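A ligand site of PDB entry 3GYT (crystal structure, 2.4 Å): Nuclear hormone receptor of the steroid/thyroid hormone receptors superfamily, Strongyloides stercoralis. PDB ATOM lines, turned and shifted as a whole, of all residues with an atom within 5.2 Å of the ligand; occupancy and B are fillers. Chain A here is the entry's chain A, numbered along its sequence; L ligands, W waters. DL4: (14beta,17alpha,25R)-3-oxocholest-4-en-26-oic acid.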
ATOM      1  N   MET A  23       7.070  22.898  -3.796  1.00  0.00           N
ATOM      2  CA  MET A  23       6.493  23.379  -2.554  1.00  0.00           C
ATOM      3  C   MET A  23       7.004  24.761  -2.208  1.00  0.00           C
ATOM      4  O   MET A  23       6.229  25.584  -1.707  1.00  0.00           O
ATOM      5  CB  MET A  23       6.796  22.449  -1.367  1.00  0.00           C
ATOM      6  CG  MET A  23       6.243  21.003  -1.463  1.00  0.00           C
ATOM      7  SD  MET A  23       4.483  20.882  -1.775  1.00  0.00           S
ATOM      8  CE  MET A  23       3.832  21.593  -0.322  1.00  0.00           C
ATOM      9  N   LEU A  36      -1.354  36.264   1.143  1.00  0.00           N
ATOM     10  CA  LEU A  36      -0.226  36.031   2.049  1.00  0.00           C
ATOM     11  C   LEU A  36       0.392  37.308   2.603  1.00  0.00           C
ATOM     12  O   LEU A  36       1.079  37.261   3.579  1.00  0.00           O
ATOM     13  CB  LEU A  36       0.872  35.229   1.358  1.00  0.00           C
ATOM     14  CG  LEU A  36       0.747  33.719   1.515  1.00  0.00           C
ATOM     15  CD1 LEU A  36       1.692  32.936   0.582  1.00  0.00           C
ATOM     16  CD2 LEU A  36       1.039  33.293   2.969  1.00  0.00           C
ATOM     17  N   ILE A  46      -7.559  32.251   5.293  1.00  0.00           N
ATOM     18  CA  ILE A  46      -6.850  31.028   5.589  1.00  0.00           C
ATOM     19  C   ILE A  46      -7.164  29.956   4.580  1.00  0.00           C
ATOM     20  O   ILE A  46      -6.355  29.148   4.265  1.00  0.00           O
ATOM     21  CB  ILE A  46      -7.144  30.505   7.016  1.00  0.00           C
ATOM     22  CG1 ILE A  46      -6.426  31.400   8.015  1.00  0.00           C
ATOM     23  CG2 ILE A  46      -6.611  29.166   7.176  1.00  0.00           C
ATOM     24  CD1 ILE A  46      -7.333  32.547   8.416  1.00  0.00           C
ATOM     25  N   VAL A  49      -5.071  30.649   1.425  1.00  0.00           N
ATOM     26  CA  VAL A  49      -3.704  30.243   1.682  1.00  0.00           C
ATOM     27  C   VAL A  49      -3.549  28.705   1.582  1.00  0.00           C
ATOM     28  O   VAL A  49      -2.596  28.226   0.991  1.00  0.00           O
ATOM     29  CB  VAL A  49      -3.273  30.631   3.029  1.00  0.00           C
ATOM     30  CG1 VAL A  49      -1.988  30.043   3.317  1.00  0.00           C
ATOM     31  CG2 VAL A  49      -3.193  32.066   3.142  1.00  0.00           C
ATOM     32  N   MET A  50      -4.483  27.942   2.144  1.00  0.00           N
ATOM     33  CA  MET A  50      -4.408  26.528   2.034  1.00  0.00           C
ATOM     34  C   MET A  50      -4.529  26.065   0.632  1.00  0.00           C
ATOM     35  O   MET A  50      -3.982  25.031   0.282  1.00  0.00           O
ATOM     36  CB  MET A  50      -5.492  25.846   2.857  1.00  0.00           C
ATOM     37  CG  MET A  50      -5.412  26.128   4.336  1.00  0.00           C
ATOM     38  SD  MET A  50      -6.724  25.289   5.270  1.00  0.00           S
ATOM     39  CE  MET A  50      -5.772  24.019   5.872  1.00  0.00           C
ATOM     40  N   ILE A  52      -3.110  27.291  -1.930  1.00  0.00           N
ATOM     41  CA  ILE A  52      -1.754  27.320  -2.472  1.00  0.00           C
ATOM     42  C   ILE A  52      -1.042  26.014  -2.143  1.00  0.00           C
ATOM     43  O   ILE A  52      -0.522  25.332  -3.040  1.00  0.00           O
ATOM     44  CB  ILE A  52      -0.932  28.394  -1.820  1.00  0.00           C
ATOM     45  CG1 ILE A  52      -1.673  29.717  -1.807  1.00  0.00           C
ATOM     46  CG2 ILE A  52       0.364  28.567  -2.557  1.00  0.00           C
ATOM     47  CD1 ILE A  52      -1.897  30.245  -3.081  1.00  0.00           C
ATOM     48  N   THR A  53      -1.021  25.664  -0.869  1.00  0.00           N
ATOM     49  CA  THR A  53      -0.317  24.458  -0.390  1.00  0.00           C
ATOM     50  C   THR A  53      -0.914  23.200  -0.922  1.00  0.00           C
ATOM     51  O   THR A  53      -0.186  22.346  -1.383  1.00  0.00           O
ATOM     52  CB  THR A  53      -0.286  24.411   1.111  1.00  0.00           C
ATOM     53  OG1 THR A  53       0.173  25.679   1.583  1.00  0.00           O
ATOM     54  CG2 THR A  53       0.653  23.334   1.563  1.00  0.00           C
ATOM     55  N   ILE A  84      -5.063  16.837   4.641  1.00  0.00           N
ATOM     56  CA  ILE A  84      -4.947  17.612   5.889  1.00  0.00           C
ATOM     57  C   ILE A  84      -3.677  17.247   6.700  1.00  0.00           C
ATOM     58  O   ILE A  84      -3.040  18.112   7.320  1.00  0.00           O
ATOM     59  CB  ILE A  84      -6.149  17.385   6.797  1.00  0.00           C
ATOM     60  CG1 ILE A  84      -7.497  17.584   6.072  1.00  0.00           C
ATOM     61  CG2 ILE A  84      -6.100  18.295   7.973  1.00  0.00           C
ATOM     62  CD1 ILE A  84      -7.672  18.863   5.541  1.00  0.00           C
ATOM     63  N   LEU A  87      -0.670  18.842   5.025  1.00  0.00           N
ATOM     64  CA  LEU A  87      -0.639  20.286   5.355  1.00  0.00           C
ATOM     65  C   LEU A  87      -0.137  20.490   6.741  1.00  0.00           C
ATOM     66  O   LEU A  87       0.657  21.450   6.964  1.00  0.00           O
ATOM     67  CB  LEU A  87      -2.003  20.931   5.290  1.00  0.00           C
ATOM     68  CG  LEU A  87      -2.619  21.210   3.943  1.00  0.00           C
ATOM     69  CD1 LEU A  87      -4.017  21.770   4.154  1.00  0.00           C
ATOM     70  CD2 LEU A  87      -1.803  22.200   3.182  1.00  0.00           C
ATOM     71  N   THR A  88      -0.619  19.654   7.684  1.00  0.00           N
ATOM     72  CA  THR A  88      -0.317  19.865   9.103  1.00  0.00           C
ATOM     73  C   THR A  88       1.173  19.693   9.262  1.00  0.00           C
ATOM     74  O   THR A  88       1.824  20.386  10.066  1.00  0.00           O
ATOM     75  CB  THR A  88      -1.034  18.875   9.972  1.00  0.00           C
ATOM     76  OG1 THR A  88      -2.433  19.018   9.803  1.00  0.00           O
ATOM     77  CG2 THR A  88      -0.678  19.072  11.389  1.00  0.00           C
ATOM     78  N   ARG A  90       3.490  20.286   6.869  1.00  0.00           N
ATOM     79  CA  ARG A  90       4.127  21.486   6.311  1.00  0.00           C
ATOM     80  C   ARG A  90       4.005  22.629   7.268  1.00  0.00           C
ATOM     81  O   ARG A  90       4.962  23.396   7.441  1.00  0.00           O
ATOM     82  CB  ARG A  90       3.543  21.868   4.953  1.00  0.00           C
ATOM     83  CG  ARG A  90       3.359  23.361   4.786  1.00  0.00           C
ATOM     84  CD  ARG A  90       3.929  24.007   3.431  1.00  0.00           C
ATOM     85  NE  ARG A  90       5.348  23.831   3.340  1.00  0.00           N
ATOM     86  CZ  ARG A  90       6.168  24.418   2.461  1.00  0.00           C
ATOM     87  NH1 ARG A  90       5.740  25.264   1.585  1.00  0.00           N
ATOM     88  NH2 ARG A  90       7.448  24.087   2.438  1.00  0.00           N
ATOM     89  N   GLY A  91       2.844  22.705   7.909  1.00  0.00           N
ATOM     90  CA  GLY A  91       2.587  23.674   8.948  1.00  0.00           C
ATOM     91  C   GLY A  91       3.618  23.668  10.038  1.00  0.00           C
ATOM     92  O   GLY A  91       4.076  24.702  10.475  1.00  0.00           O
ATOM     93  N   VAL A  94       7.230  25.155   8.899  1.00  0.00           N
ATOM     94  CA  VAL A  94       7.391  26.571   8.673  1.00  0.00           C
ATOM     95  C   VAL A  94       6.894  27.388   9.858  1.00  0.00           C
ATOM     96  O   VAL A  94       6.710  28.620   9.754  1.00  0.00           O
ATOM     97  CB  VAL A  94       6.743  27.021   7.361  1.00  0.00           C
ATOM     98  CG1 VAL A  94       7.193  26.115   6.266  1.00  0.00           C
ATOM     99  CG2 VAL A  94       5.237  27.044   7.481  1.00  0.00           C
ATOM    100  N   TRP A 102       3.252  31.421  11.384  1.00  0.00           N
ATOM    101  CA  TRP A 102       3.760  30.646  10.301  1.00  0.00           C
ATOM    102  C   TRP A 102       4.503  31.580   9.320  1.00  0.00           C
ATOM    103  O   TRP A 102       4.035  32.703   9.088  1.00  0.00           O
ATOM    104  CB  TRP A 102       2.618  29.983   9.599  1.00  0.00           C
ATOM    105  CG  TRP A 102       2.108  28.825  10.262  1.00  0.00           C
ATOM    106  CD1 TRP A 102       2.722  27.636  10.342  1.00  0.00           C
ATOM    107  CD2 TRP A 102       0.833  28.664  10.874  1.00  0.00           C
ATOM    108  NE1 TRP A 102       1.919  26.722  11.015  1.00  0.00           N
ATOM    109  CE2 TRP A 102       0.755  27.342  11.350  1.00  0.00           C
ATOM    110  CE3 TRP A 102      -0.245  29.530  11.130  1.00  0.00           C
ATOM    111  CZ2 TRP A 102      -0.354  26.847  12.034  1.00  0.00           C
ATOM    112  CZ3 TRP A 102      -1.339  29.035  11.822  1.00  0.00           C
ATOM    113  CH2 TRP A 102      -1.383  27.706  12.260  1.00  0.00           C
ATOM    114  N   THR A 104       6.085  31.416   5.528  1.00  0.00           N
ATOM    115  CA  THR A 104       6.233  30.677   4.311  1.00  0.00           C
ATOM    116  C   THR A 104       7.564  31.022   3.703  1.00  0.00           C
ATOM    117  O   THR A 104       7.885  32.172   3.534  1.00  0.00           O
ATOM    118  CB  THR A 104       5.139  31.065   3.364  1.00  0.00           C
ATOM    119  OG1 THR A 104       5.666  31.716   2.223  1.00  0.00           O
ATOM    120  CG2 THR A 104       4.157  32.042   4.068  1.00  0.00           C
ATOM    121  N   PRO A 105       8.352  30.009   3.341  1.00  0.00           N
ATOM    122  CA  PRO A 105       9.600  30.185   2.571  1.00  0.00           C
ATOM    123  C   PRO A 105       9.374  30.839   1.212  1.00  0.00           C
ATOM    124  O   PRO A 105      10.182  31.598   0.741  1.00  0.00           O
ATOM    125  CB  PRO A 105      10.095  28.744   2.369  1.00  0.00           C
ATOM    126  CG  PRO A 105       9.375  27.913   3.392  1.00  0.00           C
ATOM    127  CD  PRO A 105       8.013  28.572   3.496  1.00  0.00           C
ATOM    128  N   VAL A 106       8.263  30.547   0.573  1.00  0.00           N
ATOM    129  CA  VAL A 106       8.006  31.089  -0.713  1.00  0.00           C
ATOM    130  C   VAL A 106       7.907  32.605  -0.669  1.00  0.00           C
ATOM    131  O   VAL A 106       8.105  33.238  -1.691  1.00  0.00           O
ATOM    132  CB  VAL A 106       6.707  30.510  -1.340  1.00  0.00           C
ATOM    133  CG1 VAL A 106       5.536  30.594  -0.394  1.00  0.00           C
ATOM    134  CG2 VAL A 106       6.359  31.312  -2.541  1.00  0.00           C
ATOM    135  N   ILE A 112       1.539  34.416   9.294  1.00  0.00           N
ATOM    136  CA  ILE A 112       0.167  34.044   9.558  1.00  0.00           C
ATOM    137  C   ILE A 112       0.080  33.776  11.025  1.00  0.00           C
ATOM    138  O   ILE A 112       0.721  32.867  11.521  1.00  0.00           O
ATOM    139  CB  ILE A 112      -0.283  32.830   8.796  1.00  0.00           C
ATOM    140  CG1 ILE A 112      -0.261  33.126   7.305  1.00  0.00           C
ATOM    141  CG2 ILE A 112      -1.717  32.496   9.142  1.00  0.00           C
ATOM    142  CD1 ILE A 112      -0.498  31.986   6.486  1.00  0.00           C
ATOM    143  N   MET A 116      -5.038  32.917  14.495  1.00  0.00           N
ATOM    144  CA  MET A 116      -6.066  32.796  13.500  1.00  0.00           C
ATOM    145  C   MET A 116      -7.061  31.684  13.895  1.00  0.00           C
ATOM    146  O   MET A 116      -8.176  31.659  13.362  1.00  0.00           O
ATOM    147  CB  MET A 116      -5.461  32.527  12.108  1.00  0.00           C
ATOM    148  CG  MET A 116      -4.856  31.099  11.945  1.00  0.00           C
ATOM    149  SD  MET A 116      -6.106  29.810  11.463  1.00  0.00           S
ATOM    150  CE  MET A 116      -5.267  28.324  12.072  1.00  0.00           C
ATOM    151  N   PHE A 117      -6.667  30.819  14.823  1.00  0.00           N
ATOM    152  CA  PHE A 117      -7.540  29.713  15.346  1.00  0.00           C
ATOM    153  C   PHE A 117      -8.744  30.269  16.130  1.00  0.00           C
ATOM    154  O   PHE A 117      -9.812  29.698  16.166  1.00  0.00           O
ATOM    155  CB  PHE A 117      -6.763  28.820  16.304  1.00  0.00           C
ATOM    156  CG  PHE A 117      -6.048  27.669  15.671  1.00  0.00           C
ATOM    157  CD1 PHE A 117      -4.703  27.728  15.460  1.00  0.00           C
ATOM    158  CD2 PHE A 117      -6.726  26.501  15.318  1.00  0.00           C
ATOM    159  CE1 PHE A 117      -4.026  26.663  14.875  1.00  0.00           C
ATOM    160  CE2 PHE A 117      -6.046  25.431  14.752  1.00  0.00           C
ATOM    161  CZ  PHE A 117      -4.714  25.514  14.528  1.00  0.00           C
ATOM    162  N   LEU A 120     -11.955  30.214  14.359  1.00  0.00           N
ATOM    163  CA  LEU A 120     -12.509  28.961  13.832  1.00  0.00           C
ATOM    164  C   LEU A 120     -13.581  28.386  14.730  1.00  0.00           C
ATOM    165  O   LEU A 120     -14.009  29.046  15.649  1.00  0.00           O
ATOM    166  CB  LEU A 120     -11.380  27.977  13.602  1.00  0.00           C
ATOM    167  CG  LEU A 120     -10.278  28.524  12.661  1.00  0.00           C
ATOM    168  CD1 LEU A 120      -9.267  27.458  12.285  1.00  0.00           C
ATOM    169  CD2 LEU A 120     -10.858  29.139  11.431  1.00  0.00           C
ATOM    170  N   GLN A 128      -7.596  22.122  19.071  1.00  0.00           N
ATOM    171  CA  GLN A 128      -6.746  22.072  17.880  1.00  0.00           C
ATOM    172  C   GLN A 128      -5.439  22.799  18.084  1.00  0.00           C
ATOM    173  O   GLN A 128      -4.387  22.305  17.713  1.00  0.00           O
ATOM    174  CB  GLN A 128      -7.452  22.688  16.690  1.00  0.00           C
ATOM    175  CG  GLN A 128      -8.604  21.822  16.169  1.00  0.00           C
ATOM    176  CD  GLN A 128      -8.149  20.388  15.944  1.00  0.00           C
ATOM    177  OE1 GLN A 128      -8.421  19.516  16.713  1.00  0.00           O
ATOM    178  NE2 GLN A 128      -7.395  20.179  14.886  1.00  0.00           N
ATOM    179  N   PHE A 132      -2.023  20.957  17.593  1.00  0.00           N
ATOM    180  CA  PHE A 132      -1.007  21.357  16.631  1.00  0.00           C
ATOM    181  C   PHE A 132       0.368  21.502  17.350  1.00  0.00           C
ATOM    182  O   PHE A 132       1.412  20.980  16.859  1.00  0.00           O
ATOM    183  CB  PHE A 132      -1.359  22.646  15.880  1.00  0.00           C
ATOM    184  CG  PHE A 132      -0.277  23.093  14.939  1.00  0.00           C
ATOM    185  CD1 PHE A 132      -0.166  22.560  13.704  1.00  0.00           C
ATOM    186  CD2 PHE A 132       0.654  23.991  15.335  1.00  0.00           C
ATOM    187  CE1 PHE A 132       0.893  22.931  12.821  1.00  0.00           C
ATOM    188  CE2 PHE A 132       1.689  24.361  14.497  1.00  0.00           C
ATOM    189  CZ  PHE A 132       1.813  23.810  13.224  1.00  0.00           C
ATOM    190  N   VAL A 215      -4.844  15.059  15.448  1.00  0.00           N
ATOM    191  CA  VAL A 215      -5.067  16.477  15.208  1.00  0.00           C
ATOM    192  C   VAL A 215      -5.713  16.739  13.882  1.00  0.00           C
ATOM    193  O   VAL A 215      -6.681  17.523  13.832  1.00  0.00           O
ATOM    194  CB  VAL A 215      -3.783  17.246  15.207  1.00  0.00           C
ATOM    195  CG1 VAL A 215      -4.067  18.756  15.205  1.00  0.00           C
ATOM    196  CG2 VAL A 215      -3.017  16.884  16.418  1.00  0.00           C
ATOM    197  N   ALA A 219      -9.887  18.215  12.592  1.00  0.00           N
ATOM    198  CA  ALA A 219      -9.702  19.551  12.062  1.00  0.00           C
ATOM    199  C   ALA A 219     -10.652  19.816  10.929  1.00  0.00           C
ATOM    200  O   ALA A 219     -10.759  20.969  10.493  1.00  0.00           O
ATOM    201  CB  ALA A 219      -8.370  19.716  11.577  1.00  0.00           C
ATOM    202  N   LEU A 222     -13.324  22.660  11.400  1.00  0.00           N
ATOM    203  CA  LEU A 222     -12.825  23.917  12.020  1.00  0.00           C
ATOM    204  C   LEU A 222     -13.454  25.134  11.398  1.00  0.00           C
ATOM    205  O   LEU A 222     -13.453  26.177  12.011  1.00  0.00           O
ATOM    206  CB  LEU A 222     -11.316  24.081  11.892  1.00  0.00           C
ATOM    207  CG  LEU A 222     -10.449  23.599  13.049  1.00  0.00           C
ATOM    208  CD1 LEU A 222      -8.983  23.638  12.669  1.00  0.00           C
ATOM    209  CD2 LEU A 222     -10.685  24.488  14.295  1.00  0.00           C
ATOM    210  N   PHE A 240     -12.616  20.535   3.905  1.00  0.00           N
ATOM    211  CA  PHE A 240     -13.119  21.161   5.139  1.00  0.00           C
ATOM    212  C   PHE A 240     -14.584  21.397   5.033  1.00  0.00           C
ATOM    213  O   PHE A 240     -15.031  21.993   4.059  1.00  0.00           O
ATOM    214  CB  PHE A 240     -12.418  22.497   5.425  1.00  0.00           C
ATOM    215  CG  PHE A 240     -11.000  22.353   5.892  1.00  0.00           C
ATOM    216  CD1 PHE A 240     -10.730  22.159   7.239  1.00  0.00           C
ATOM    217  CD2 PHE A 240      -9.946  22.342   4.971  1.00  0.00           C
ATOM    218  CE1 PHE A 240      -9.436  21.971   7.694  1.00  0.00           C
ATOM    219  CE2 PHE A 240      -8.653  22.145   5.404  1.00  0.00           C
ATOM    220  CZ  PHE A 240      -8.375  21.994   6.759  1.00  0.00           C
HETATM  221  O3  DL4 L   1       4.070  28.520   1.889  1.00  0.00           O
HETATM  222  C27 DL4 L   1       3.097  27.764   2.116  1.00  0.00           C
HETATM  223  O2  DL4 L   1       3.176  26.518   2.160  1.00  0.00           O
HETATM  224  C25 DL4 L   1       1.742  28.349   2.368  1.00  0.00           C
HETATM  225  C26 DL4 L   1       1.328  29.032   1.108  1.00  0.00           C
HETATM  226  C24 DL4 L   1       1.706  29.242   3.594  1.00  0.00           C
HETATM  227  C23 DL4 L   1       2.205  28.534   4.857  1.00  0.00           C
HETATM  228  C22 DL4 L   1       1.141  28.467   5.958  1.00  0.00           C
HETATM  229  C20 DL4 L   1       0.468  27.081   6.103  1.00  0.00           C
HETATM  230  C21 DL4 L   1       1.587  26.108   6.449  1.00  0.00           C
HETATM  231  C17 DL4 L   1      -0.618  27.095   7.196  1.00  0.00           C
HETATM  232  C16 DL4 L   1      -1.706  28.148   6.927  1.00  0.00           C
HETATM  233  C15 DL4 L   1      -3.054  27.669   7.505  1.00  0.00           C
HETATM  234  C14 DL4 L   1      -2.581  26.471   8.312  1.00  0.00           C
HETATM  235  C8  DL4 L   1      -3.516  25.333   8.753  1.00  0.00           C
HETATM  236  C7  DL4 L   1      -4.745  25.877   9.485  1.00  0.00           C
HETATM  237  C6  DL4 L   1      -5.828  24.835   9.848  1.00  0.00           C
HETATM  238  C13 DL4 L   1      -1.416  25.854   7.541  1.00  0.00           C
HETATM  239  C18 DL4 L   1      -1.971  25.185   6.270  1.00  0.00           C
HETATM  240  C12 DL4 L   1      -0.747  24.847   8.456  1.00  0.00           C
HETATM  241  C11 DL4 L   1      -1.706  23.706   8.869  1.00  0.00           C
HETATM  242  C9  DL4 L   1      -3.004  24.156   9.558  1.00  0.00           C
HETATM  243  C10 DL4 L   1      -3.981  23.042   9.970  1.00  0.00           C
HETATM  244  C1  DL4 L   1      -3.240  22.242  11.007  1.00  0.00           C
HETATM  245  C19 DL4 L   1      -4.376  22.193   8.768  1.00  0.00           C
HETATM  246  C5  DL4 L   1      -5.223  23.661  10.577  1.00  0.00           C
HETATM  247  C4  DL4 L   1      -5.801  23.251  11.700  1.00  0.00           C
HETATM  248  C3  DL4 L   1      -5.316  22.092  12.420  1.00  0.00           C
HETATM  249  O1  DL4 L   1      -5.879  21.677  13.403  1.00  0.00           O
HETATM  250  C2  DL4 L   1      -4.112  21.376  11.910  1.00  0.00           C
HETATM  251  O   HOH W   1       3.388  25.236  -0.340  1.00  0.00           O
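CD1 of Leu 36 touches C26 of the ligand, 3.96 Å away.
Ile 46 touches the ligand.
Val 49 touches the ligand.
CE of Met 50 touches C19 of the ligand, 3.7 Å away.
CB of Ile 52 touches C26 of the ligand (3.8 Å).
O of Leu 87 touches C11 of the ligand, 3.8 Å away.
OG1 of Thr 88 touches C1 of the ligand, at 3.5 Å.
Gly 91 touches the ligand.
Val 94 touches the ligand.
CB of Thr 104 touches O3 of the ligand, 3.1 Å away.
Val 106 touches the ligand (CG1 to O3, 3.4 Å).
Ile 112 touches the ligand.
Met 116 touches the ligand (CE to C7, 3.6 Å).
Phe 117 touches the ligand.
CG1 of Val 215 touches O1 of the ligand (3.9 Å).
Ala 219 touches the ligand (CB to O1, 3.7 Å).
Leu 222 touches the ligand.
Hydrophobic or aromatic side chains within 4 Å of the ligand: Leu 36, Ile 46, Val 49, Met 50, Ile 52, Val 94, Val 106, Ile 112, Met 116, Phe 117, Val 215, Ala 219 and Leu 222.
20 residues have an atom within 4 Å of the ligand: Leu 36, Ile 46, Val 49, Met 50, Ile 52, Thr 53, Leu 87, Thr 88, Arg 90, Gly 91, Val 94, Thr 104, Val 106, Ile 112, Met 116, Phe 117, Gln 128, Val 215, Ala 219 and Leu 222.
The backbone carbonyl oxygen of Ile 112 is in hydrogen-bond range of the backbone NH of Trp 102, 2.9 Å away.
The indole nitrogen of Trp 102 is in hydrogen-bond range of the backbone carbonyl oxygen of Gly 91.
O of Ile 84 is in hydrogen-bond range of OG1 of Thr 88.
The guanidinium group (NH1) of Arg 90 sits at hydrogen-bond distance from the backbone carbonyl oxygen (O) of Met 23 (3.3 Å).
The side-chain hydroxyl (OG1) of Thr 104 lies close to the backbone NH (N) of Val 106 (3.3 Å).
The backbone carbonyl oxygen of Val 215 is in hydrogen-bond range of the side-chain amide nitrogen of Gln 128, at 2.9 Å.
Water W1 lies within hydrogen-bond range of an oxygen (O2) of the ligand (2.8 Å), the guanidinium group (NH1) of Arg 90 (3.0 Å) and the backbone carbonyl oxygen (O) of Met 23 (3.2 Å).
O1 of the ligand sits at hydrogen-bond distance from NE2 of Gln 128 (2.6 Å).
The guanidinium group of Arg 90 is in salt-bridge range of an oxygen (O2) of the ligand.
The side-chain hydroxyl (OG1) of Thr 53 is in hydrogen-bond range of an oxygen (O2) of the ligand (3.2 Å).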
